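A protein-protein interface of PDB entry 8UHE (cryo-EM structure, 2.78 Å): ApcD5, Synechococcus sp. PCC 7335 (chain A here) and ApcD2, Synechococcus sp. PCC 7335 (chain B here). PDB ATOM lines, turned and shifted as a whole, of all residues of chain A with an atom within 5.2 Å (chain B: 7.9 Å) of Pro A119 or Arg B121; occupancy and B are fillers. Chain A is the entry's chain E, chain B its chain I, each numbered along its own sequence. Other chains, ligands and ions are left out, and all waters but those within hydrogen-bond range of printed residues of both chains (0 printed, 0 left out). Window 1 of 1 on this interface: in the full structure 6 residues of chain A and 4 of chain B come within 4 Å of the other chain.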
ATOM      1  N   PRO A  66      25.326 -21.810  22.013  1.00  0.00           N
ATOM      2  CA  PRO A  66      25.011 -23.247  22.004  1.00  0.00           C
ATOM      3  C   PRO A  66      26.245 -24.132  21.994  1.00  0.00           C
ATOM      4  O   PRO A  66      26.140 -25.315  22.336  1.00  0.00           O
ATOM      5  CB  PRO A  66      24.183 -23.421  20.722  1.00  0.00           C
ATOM      6  CG  PRO A  66      23.654 -22.062  20.420  1.00  0.00           C
ATOM      7  CD  PRO A  66      24.689 -21.096  20.892  1.00  0.00           C
ATOM      8  N   TYR A 113      22.059 -20.991   9.242  1.00  0.00           N
ATOM      9  CA  TYR A 113      22.399 -20.910  10.655  1.00  0.00           C
ATOM     10  C   TYR A 113      21.328 -20.207  11.479  1.00  0.00           C
ATOM     11  O   TYR A 113      21.332 -20.341  12.708  1.00  0.00           O
ATOM     12  CB  TYR A 113      23.753 -20.226  10.822  1.00  0.00           C
ATOM     13  CG  TYR A 113      24.915 -21.194  10.898  1.00  0.00           C
ATOM     14  CD1 TYR A 113      24.869 -22.300  11.733  1.00  0.00           C
ATOM     15  CD2 TYR A 113      26.057 -20.999  10.132  1.00  0.00           C
ATOM     16  CE1 TYR A 113      25.930 -23.187  11.807  1.00  0.00           C
ATOM     17  CE2 TYR A 113      27.120 -21.875  10.200  1.00  0.00           C
ATOM     18  CZ  TYR A 113      27.052 -22.967  11.039  1.00  0.00           C
ATOM     19  OH  TYR A 113      28.115 -23.837  11.101  1.00  0.00           O
ATOM     20  N   ASN A 114      20.416 -19.468  10.843  1.00  0.00           N
ATOM     21  CA  ASN A 114      19.196 -19.043  11.514  1.00  0.00           C
ATOM     22  C   ASN A 114      18.241 -20.209  11.682  1.00  0.00           C
ATOM     23  O   ASN A 114      17.577 -20.327  12.714  1.00  0.00           O
ATOM     24  CB  ASN A 114      18.516 -17.929  10.724  1.00  0.00           C
ATOM     25  CG  ASN A 114      18.961 -16.558  11.155  1.00  0.00           C
ATOM     26  OD1 ASN A 114      20.116 -16.181  10.969  1.00  0.00           O
ATOM     27  ND2 ASN A 114      18.045 -15.796  11.738  1.00  0.00           N
ATOM     28  N   GLU A 117      18.953 -22.049  14.528  1.00  0.00           N
ATOM     29  CA  GLU A 117      18.736 -21.179  15.682  1.00  0.00           C
ATOM     30  C   GLU A 117      20.036 -20.744  16.343  1.00  0.00           C
ATOM     31  O   GLU A 117      20.050 -20.405  17.531  1.00  0.00           O
ATOM     32  CB  GLU A 117      17.787 -21.812  16.714  1.00  0.00           C
ATOM     33  CG  GLU A 117      16.317 -22.062  16.265  1.00  0.00           C
ATOM     34  CD  GLU A 117      15.787 -21.209  15.096  1.00  0.00           C
ATOM     35  OE1 GLU A 117      16.007 -19.977  15.028  1.00  0.00           O
ATOM     36  OE2 GLU A 117      15.119 -21.791  14.220  1.00  0.00           O
ATOM     37  N   ILE A 118      21.118 -20.710  15.581  1.00  0.00           N
ATOM     38  CA  ILE A 118      22.414 -20.275  16.097  1.00  0.00           C
ATOM     39  C   ILE A 118      22.567 -18.778  15.843  1.00  0.00           C
ATOM     40  O   ILE A 118      22.305 -18.322  14.718  1.00  0.00           O
ATOM     41  CB  ILE A 118      23.534 -21.067  15.437  1.00  0.00           C
ATOM     42  CG1 ILE A 118      23.378 -22.545  15.796  1.00  0.00           C
ATOM     43  CG2 ILE A 118      24.897 -20.541  15.846  1.00  0.00           C
ATOM     44  CD1 ILE A 118      24.321 -23.439  15.080  1.00  0.00           C
ATOM     45  N   PRO A 119      22.940 -17.989  16.853  1.00  0.00           N
ATOM     46  CA  PRO A 119      23.158 -16.553  16.628  1.00  0.00           C
ATOM     47  C   PRO A 119      24.313 -16.314  15.666  1.00  0.00           C
ATOM     48  O   PRO A 119      25.404 -16.859  15.833  1.00  0.00           O
ATOM     49  CB  PRO A 119      23.474 -16.014  18.028  1.00  0.00           C
ATOM     50  CG  PRO A 119      23.008 -17.063  18.980  1.00  0.00           C
ATOM     51  CD  PRO A 119      23.111 -18.370  18.264  1.00  0.00           C
ATOM     52  N   ILE A 120      24.055 -15.475  14.659  1.00  0.00           N
ATOM     53  CA  ILE A 120      25.004 -15.273  13.565  1.00  0.00           C
ATOM     54  C   ILE A 120      26.266 -14.570  14.061  1.00  0.00           C
ATOM     55  O   ILE A 120      27.390 -14.929  13.676  1.00  0.00           O
ATOM     56  CB  ILE A 120      24.315 -14.495  12.427  1.00  0.00           C
ATOM     57  CG1 ILE A 120      23.333 -15.401  11.683  1.00  0.00           C
ATOM     58  CG2 ILE A 120      25.322 -13.938  11.445  1.00  0.00           C
ATOM     59  CD1 ILE A 120      23.993 -16.563  10.994  1.00  0.00           C
ATOM     60  N   ARG A 121      26.106 -13.576  14.937  1.00  0.00           N
ATOM     61  CA  ARG A 121      27.255 -12.822  15.421  1.00  0.00           C
ATOM     62  C   ARG A 121      28.164 -13.655  16.311  1.00  0.00           C
ATOM     63  O   ARG A 121      29.356 -13.350  16.418  1.00  0.00           O
ATOM     64  CB  ARG A 121      26.789 -11.579  16.167  1.00  0.00           C
ATOM     65  CG  ARG A 121      26.794 -10.341  15.301  1.00  0.00           C
ATOM     66  CD  ARG A 121      28.231  -9.878  14.991  1.00  0.00           C
ATOM     67  NE  ARG A 121      29.124  -9.700  16.139  1.00  0.00           N
ATOM     68  CZ  ARG A 121      28.872  -9.016  17.252  1.00  0.00           C
ATOM     69  NH1 ARG A 121      27.802  -8.277  17.388  1.00  0.00           N
ATOM     70  NH2 ARG A 121      29.753  -9.038  18.242  1.00  0.00           N
ATOM     71  N   ASN A 122      27.630 -14.708  16.931  1.00  0.00           N
ATOM     72  CA  ASN A 122      28.473 -15.650  17.657  1.00  0.00           C
ATOM     73  C   ASN A 122      29.400 -16.395  16.704  1.00  0.00           C
ATOM     74  O   ASN A 122      30.590 -16.575  16.993  1.00  0.00           O
ATOM     75  CB  ASN A 122      27.598 -16.629  18.438  1.00  0.00           C
ATOM     76  CG  ASN A 122      26.877 -15.971  19.603  1.00  0.00           C
ATOM     77  OD1 ASN A 122      26.060 -16.604  20.270  1.00  0.00           O
ATOM     78  ND2 ASN A 122      27.183 -14.703  19.863  1.00  0.00           N
ATOM     79  N   ILE A 123      28.877 -16.811  15.549  1.00  0.00           N
ATOM     80  CA  ILE A 123      29.714 -17.453  14.540  1.00  0.00           C
ATOM     81  C   ILE A 123      30.733 -16.467  13.994  1.00  0.00           C
ATOM     82  O   ILE A 123      31.863 -16.842  13.672  1.00  0.00           O
ATOM     83  CB  ILE A 123      28.853 -18.046  13.411  1.00  0.00           C
ATOM     84  CG1 ILE A 123      27.466 -18.398  13.930  1.00  0.00           C
ATOM     85  CG2 ILE A 123      29.522 -19.288  12.842  1.00  0.00           C
ATOM     86  CD1 ILE A 123      26.493 -18.746  12.846  1.00  0.00           C
ATOM     87  N   PHE B  58       9.228 -11.296  30.037  1.00  0.00           N
ATOM     88  CA  PHE B  58      10.291 -11.412  29.047  1.00  0.00           C
ATOM     89  C   PHE B  58      11.648 -11.585  29.714  1.00  0.00           C
ATOM     90  O   PHE B  58      12.468 -12.393  29.267  1.00  0.00           O
ATOM     91  CB  PHE B  58      10.256 -10.171  28.150  1.00  0.00           C
ATOM     92  CG  PHE B  58      11.467  -9.988  27.279  1.00  0.00           C
ATOM     93  CD1 PHE B  58      11.914 -11.000  26.442  1.00  0.00           C
ATOM     94  CD2 PHE B  58      12.136  -8.776  27.271  1.00  0.00           C
ATOM     95  CE1 PHE B  58      13.018 -10.808  25.638  1.00  0.00           C
ATOM     96  CE2 PHE B  58      13.236  -8.579  26.468  1.00  0.00           C
ATOM     97  CZ  PHE B  58      13.675  -9.594  25.650  1.00  0.00           C
ATOM     98  N   CYS B  62      13.926 -14.701  29.390  1.00  0.00           N
ATOM     99  CA  CYS B  62      15.107 -14.371  28.599  1.00  0.00           C
ATOM    100  C   CYS B  62      15.988 -13.390  29.363  1.00  0.00           C
ATOM    101  O   CYS B  62      16.005 -12.195  29.041  1.00  0.00           O
ATOM    102  CB  CYS B  62      14.706 -13.774  27.249  1.00  0.00           C
ATOM    103  SG  CYS B  62      15.978 -13.895  25.969  1.00  0.00           S
ATOM    104  N   THR B  65      19.724 -10.480  27.856  1.00  0.00           N
ATOM    105  CA  THR B  65      19.223  -9.540  26.868  1.00  0.00           C
ATOM    106  C   THR B  65      19.830  -8.173  27.136  1.00  0.00           C
ATOM    107  O   THR B  65      20.231  -7.884  28.270  1.00  0.00           O
ATOM    108  CB  THR B  65      17.689  -9.436  26.903  1.00  0.00           C
ATOM    109  OG1 THR B  65      17.225  -9.545  28.255  1.00  0.00           O
ATOM    110  CG2 THR B  65      17.068 -10.512  26.054  1.00  0.00           C
ATOM    111  N   TYR B 113      16.885  -4.124  13.427  1.00  0.00           N
ATOM    112  CA  TYR B 113      17.414  -4.810  14.596  1.00  0.00           C
ATOM    113  C   TYR B 113      18.680  -5.594  14.282  1.00  0.00           C
ATOM    114  O   TYR B 113      19.461  -5.870  15.197  1.00  0.00           O
ATOM    115  CB  TYR B 113      16.353  -5.725  15.188  1.00  0.00           C
ATOM    116  CG  TYR B 113      15.362  -5.021  16.084  1.00  0.00           C
ATOM    117  CD1 TYR B 113      15.788  -4.280  17.179  1.00  0.00           C
ATOM    118  CD2 TYR B 113      14.000  -5.102  15.838  1.00  0.00           C
ATOM    119  CE1 TYR B 113      14.884  -3.643  18.003  1.00  0.00           C
ATOM    120  CE2 TYR B 113      13.091  -4.468  16.654  1.00  0.00           C
ATOM    121  CZ  TYR B 113      13.535  -3.742  17.732  1.00  0.00           C
ATOM    122  OH  TYR B 113      12.618  -3.113  18.539  1.00  0.00           O
ATOM    123  N   GLU B 117      21.978  -4.848  16.127  1.00  0.00           N
ATOM    124  CA  GLU B 117      22.526  -6.102  16.652  1.00  0.00           C
ATOM    125  C   GLU B 117      21.632  -6.719  17.726  1.00  0.00           C
ATOM    126  O   GLU B 117      21.971  -7.757  18.302  1.00  0.00           O
ATOM    127  CB  GLU B 117      23.961  -5.904  17.170  1.00  0.00           C
ATOM    128  CG  GLU B 117      24.845  -7.124  17.006  1.00  0.00           C
ATOM    129  CD  GLU B 117      25.001  -7.921  18.295  1.00  0.00           C
ATOM    130  OE1 GLU B 117      24.551  -7.437  19.347  1.00  0.00           O
ATOM    131  OE2 GLU B 117      25.580  -9.034  18.246  1.00  0.00           O
ATOM    132  N   VAL B 118      20.469  -6.125  17.972  1.00  0.00           N
ATOM    133  CA  VAL B 118      19.502  -6.653  18.930  1.00  0.00           C
ATOM    134  C   VAL B 118      18.960  -7.967  18.379  1.00  0.00           C
ATOM    135  O   VAL B 118      18.473  -7.999  17.240  1.00  0.00           O
ATOM    136  CB  VAL B 118      18.376  -5.640  19.192  1.00  0.00           C
ATOM    137  CG1 VAL B 118      17.421  -6.158  20.249  1.00  0.00           C
ATOM    138  CG2 VAL B 118      18.957  -4.294  19.597  1.00  0.00           C
ATOM    139  N   PRO B 119      19.053  -9.066  19.130  1.00  0.00           N
ATOM    140  CA  PRO B 119      18.636 -10.377  18.602  1.00  0.00           C
ATOM    141  C   PRO B 119      17.139 -10.422  18.334  1.00  0.00           C
ATOM    142  O   PRO B 119      16.323 -10.164  19.220  1.00  0.00           O
ATOM    143  CB  PRO B 119      19.045 -11.349  19.714  1.00  0.00           C
ATOM    144  CG  PRO B 119      20.110 -10.624  20.478  1.00  0.00           C
ATOM    145  CD  PRO B 119      19.711  -9.186  20.441  1.00  0.00           C
ATOM    146  N   LEU B 120      16.788 -10.754  17.090  1.00  0.00           N
ATOM    147  CA  LEU B 120      15.390 -10.722  16.677  1.00  0.00           C
ATOM    148  C   LEU B 120      14.589 -11.853  17.305  1.00  0.00           C
ATOM    149  O   LEU B 120      13.367 -11.734  17.450  1.00  0.00           O
ATOM    150  CB  LEU B 120      15.297 -10.778  15.157  1.00  0.00           C
ATOM    151  CG  LEU B 120      15.675  -9.458  14.493  1.00  0.00           C
ATOM    152  CD1 LEU B 120      16.416  -9.702  13.197  1.00  0.00           C
ATOM    153  CD2 LEU B 120      14.428  -8.632  14.260  1.00  0.00           C
ATOM    154  N   ARG B 121      15.251 -12.951  17.675  1.00  0.00           N
ATOM    155  CA  ARG B 121      14.578 -13.982  18.454  1.00  0.00           C
ATOM    156  C   ARG B 121      14.183 -13.452  19.825  1.00  0.00           C
ATOM    157  O   ARG B 121      13.120 -13.797  20.351  1.00  0.00           O
ATOM    158  CB  ARG B 121      15.472 -15.213  18.592  1.00  0.00           C
ATOM    159  CG  ARG B 121      15.899 -15.817  17.270  1.00  0.00           C
ATOM    160  CD  ARG B 121      16.453 -17.223  17.447  1.00  0.00           C
ATOM    161  NE  ARG B 121      17.205 -17.643  16.272  1.00  0.00           N
ATOM    162  CZ  ARG B 121      18.528 -17.644  16.189  1.00  0.00           C
ATOM    163  NH1 ARG B 121      19.286 -17.326  17.227  1.00  0.00           N
ATOM    164  NH2 ARG B 121      19.106 -17.963  15.035  1.00  0.00           N
ATOM    165  N   SER B 122      15.024 -12.597  20.412  1.00  0.00           N
ATOM    166  CA  SER B 122      14.696 -12.002  21.703  1.00  0.00           C
ATOM    167  C   SER B 122      13.523 -11.031  21.588  1.00  0.00           C
ATOM    168  O   SER B 122      12.664 -10.985  22.476  1.00  0.00           O
ATOM    169  CB  SER B 122      15.928 -11.309  22.280  1.00  0.00           C
ATOM    170  OG  SER B 122      17.005 -12.216  22.423  1.00  0.00           O
ATOM    171  N   VAL B 123      13.459 -10.260  20.497  1.00  0.00           N
ATOM    172  CA  VAL B 123      12.302  -9.396  20.259  1.00  0.00           C
ATOM    173  C   VAL B 123      11.050 -10.234  20.029  1.00  0.00           C
ATOM    174  O   VAL B 123       9.949  -9.865  20.456  1.00  0.00           O
ATOM    175  CB  VAL B 123      12.557  -8.448  19.072  1.00  0.00           C
ATOM    176  CG1 VAL B 123      11.584  -7.281  19.108  1.00  0.00           C
ATOM    177  CG2 VAL B 123      13.979  -7.945  19.080  1.00  0.00           C
ATOM    178  N   ALA B 124      11.199 -11.370  19.344  1.00  0.00           N
ATOM    179  CA  ALA B 124      10.063 -12.254  19.107  1.00  0.00           C
ATOM    180  C   ALA B 124       9.557 -12.863  20.406  1.00  0.00           C
ATOM    181  O   ALA B 124       8.346 -13.004  20.607  1.00  0.00           O
ATOM    182  CB  ALA B 124      10.451 -13.346  18.112  1.00  0.00           C
ATOM    183  N   LEU B 125      10.474 -13.219  21.305  1.00  0.00           N
ATOM    184  CA  LEU B 125      10.086 -13.730  22.615  1.00  0.00           C
ATOM    185  C   LEU B 125       9.419 -12.652  23.461  1.00  0.00           C
ATOM    186  O   LEU B 125       8.465 -12.934  24.200  1.00  0.00           O
ATOM    187  CB  LEU B 125      11.308 -14.289  23.334  1.00  0.00           C
ATOM    188  CG  LEU B 125      11.056 -15.524  24.190  1.00  0.00           C
ATOM    189  CD1 LEU B 125      10.995 -16.767  23.321  1.00  0.00           C
ATOM    190  CD2 LEU B 125      12.143 -15.640  25.238  1.00  0.00           C
ATOM    191  N   CYS B 126       9.922 -11.415  23.384  1.00  0.00           N
ATOM    192  CA  CYS B 126       9.278 -10.320  24.102  1.00  0.00           C
ATOM    193  C   CYS B 126       7.870 -10.085  23.580  1.00  0.00           C
ATOM    194  O   CYS B 126       6.942  -9.868  24.362  1.00  0.00           O
ATOM    195  CB  CYS B 126      10.102  -9.041  23.990  1.00  0.00           C
ATOM    196  SG  CYS B 126       9.128  -7.552  24.258  1.00  0.00           S
ATOM    197  N   MET B 127       7.685 -10.153  22.262  1.00  0.00           N
ATOM    198  CA  MET B 127       6.345 -10.001  21.712  1.00  0.00           C
ATOM    199  C   MET B 127       5.460 -11.202  22.034  1.00  0.00           C
ATOM    200  O   MET B 127       4.243 -11.046  22.154  1.00  0.00           O
ATOM    201  CB  MET B 127       6.424  -9.759  20.208  1.00  0.00           C
ATOM    202  CG  MET B 127       6.992  -8.402  19.827  1.00  0.00           C
ATOM    203  SD  MET B 127       6.821  -7.158  21.120  1.00  0.00           S
ATOM    204  CE  MET B 127       8.393  -6.314  20.968  1.00  0.00           C
ATOM    205  N   ARG B 128       6.046 -12.392  22.203  1.00  0.00           N
ATOM    206  CA  ARG B 128       5.298 -13.540  22.717  1.00  0.00           C
ATOM    207  C   ARG B 128       4.771 -13.275  24.124  1.00  0.00           C
ATOM    208  O   ARG B 128       3.594 -13.526  24.424  1.00  0.00           O
ATOM    209  CB  ARG B 128       6.190 -14.784  22.718  1.00  0.00           C
ATOM    210  CG  ARG B 128       5.573 -16.037  22.120  1.00  0.00           C
ATOM    211  CD  ARG B 128       5.982 -16.250  20.671  1.00  0.00           C
ATOM    212  NE  ARG B 128       7.413 -16.512  20.546  1.00  0.00           N
ATOM    213  CZ  ARG B 128       8.051 -16.678  19.395  1.00  0.00           C
ATOM    214  NH1 ARG B 128       7.405 -16.752  18.261  1.00  0.00           N
ATOM    215  NH2 ARG B 128       9.364 -16.853  19.392  1.00  0.00           N
ATOM    216  N   ILE B 154       5.055 -11.077  15.531  1.00  0.00           N
ATOM    217  CA  ILE B 154       6.100 -12.023  15.905  1.00  0.00           C
ATOM    218  C   ILE B 154       6.714 -12.653  14.662  1.00  0.00           C
ATOM    219  O   ILE B 154       7.940 -12.672  14.496  1.00  0.00           O
ATOM    220  CB  ILE B 154       5.538 -13.088  16.857  1.00  0.00           C
ATOM    221  CG1 ILE B 154       5.250 -12.491  18.232  1.00  0.00           C
ATOM    222  CG2 ILE B 154       6.499 -14.151  16.973  1.00  0.00           C
ATOM    223  CD1 ILE B 154       4.256 -13.274  19.053  1.00  0.00           C
ATOM    224  N   LEU B 157       9.458 -11.027  12.631  1.00  0.00           N
ATOM    225  CA  LEU B 157      10.825 -11.083  13.127  1.00  0.00           C
ATOM    226  C   LEU B 157      11.230 -12.467  13.610  1.00  0.00           C
ATOM    227  O   LEU B 157      12.402 -12.667  13.950  1.00  0.00           O
ATOM    228  CB  LEU B 157      11.023 -10.069  14.263  1.00  0.00           C
ATOM    229  CG  LEU B 157       9.751  -9.490  14.881  1.00  0.00           C
ATOM    230  CD1 LEU B 157       9.462 -10.137  16.209  1.00  0.00           C
ATOM    231  CD2 LEU B 157       9.872  -7.988  15.047  1.00  0.00           C
ATOM    232  N   MET B 158      10.311 -13.403  13.475  1.00  0.00           N
ATOM    233  CA  MET B 158      10.654 -14.714  13.947  1.00  0.00           C
ATOM    234  C   MET B 158      11.838 -15.255  13.151  1.00  0.00           C
ATOM    235  O   MET B 158      12.416 -16.265  13.544  1.00  0.00           O
ATOM    236  CB  MET B 158       9.446 -15.661  13.936  1.00  0.00           C
ATOM    237  CG  MET B 158       9.504 -16.723  15.021  1.00  0.00           C
ATOM    238  SD  MET B 158      11.085 -16.748  15.887  1.00  0.00           S
ATOM    239  CE  MET B 158      11.488 -18.490  15.783  1.00  0.00           C
ATOM    240  N   PRO B 159      12.244 -14.586  12.069  1.00  0.00           N
ATOM    241  CA  PRO B 159      13.442 -15.142  11.430  1.00  0.00           C
ATOM    242  C   PRO B 159      14.768 -14.655  11.968  1.00  0.00           C
ATOM    243  O   PRO B 159      15.078 -14.883  13.136  1.00  0.00           O
ATOM    244  CB  PRO B 159      13.282 -14.738   9.942  1.00  0.00           C
ATOM    245  CG  PRO B 159      12.295 -13.633   9.938  1.00  0.00           C
ATOM    246  CD  PRO B 159      11.370 -13.934  11.069  1.00  0.00           C
ATOM    247  OXT PRO B 159      15.564 -14.099  11.198  1.00  0.00           O
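N of Ile A118 is in hydrogen-bond range of O of Tyr A113.
Printed residues of chain B within 4 Å of Asn A114: Arg B121 and Pro B159. Of the printed residues of chain B, Glu A117 touches Arg B121. Pro A119 touches just one residue of chain B: Arg B121. Printed residues of chain A within 4 Å of Arg B121: Asn A114 (3.6 Å), Glu A117 (2.9 Å), Ile A118 (3.2 Å) and Pro A119 (3.7 Å). Ile B154 touches none of the printed residues of chain A.
Among the printed residues, pairs that only touch across the chains: Asn A114 with Arg B121 (3.6 Å) and Pro A119 with Arg B121 (3.7 Å).
Of the 10 printed residues of chain A, 5 touch a printed residue of chain B. Printed residues of chain A that touch a printed residue of chain B: Asn A114, Glu A117, Ile A118, Pro A119 and Arg A121. Along chain A the printed residues that touch a printed residue of chain B span positions 114 to 121. Printed residues of chain B that touch a printed residue of chain A: Glu B117, Arg B121 and Pro B159.
OXT of Pro B159 lies within hydrogen-bond range of ND2 of Asn A114, 3.1 Å away. The side-chain carboxylate (OE1) of Glu A117 is in salt-bridge range of the guanidinium group (NE) of Arg B121 (2.9 Å). The backbone carbonyl oxygen (O) of Ile A118 lies within hydrogen-bond range of the guanidinium group (NH2) of Arg B121 (3.2 Å). The guanidinium group (NH1) of Arg A121 is in salt-bridge range of the side-chain carboxylate (OE2) of Glu B117, at 2.5 Å.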
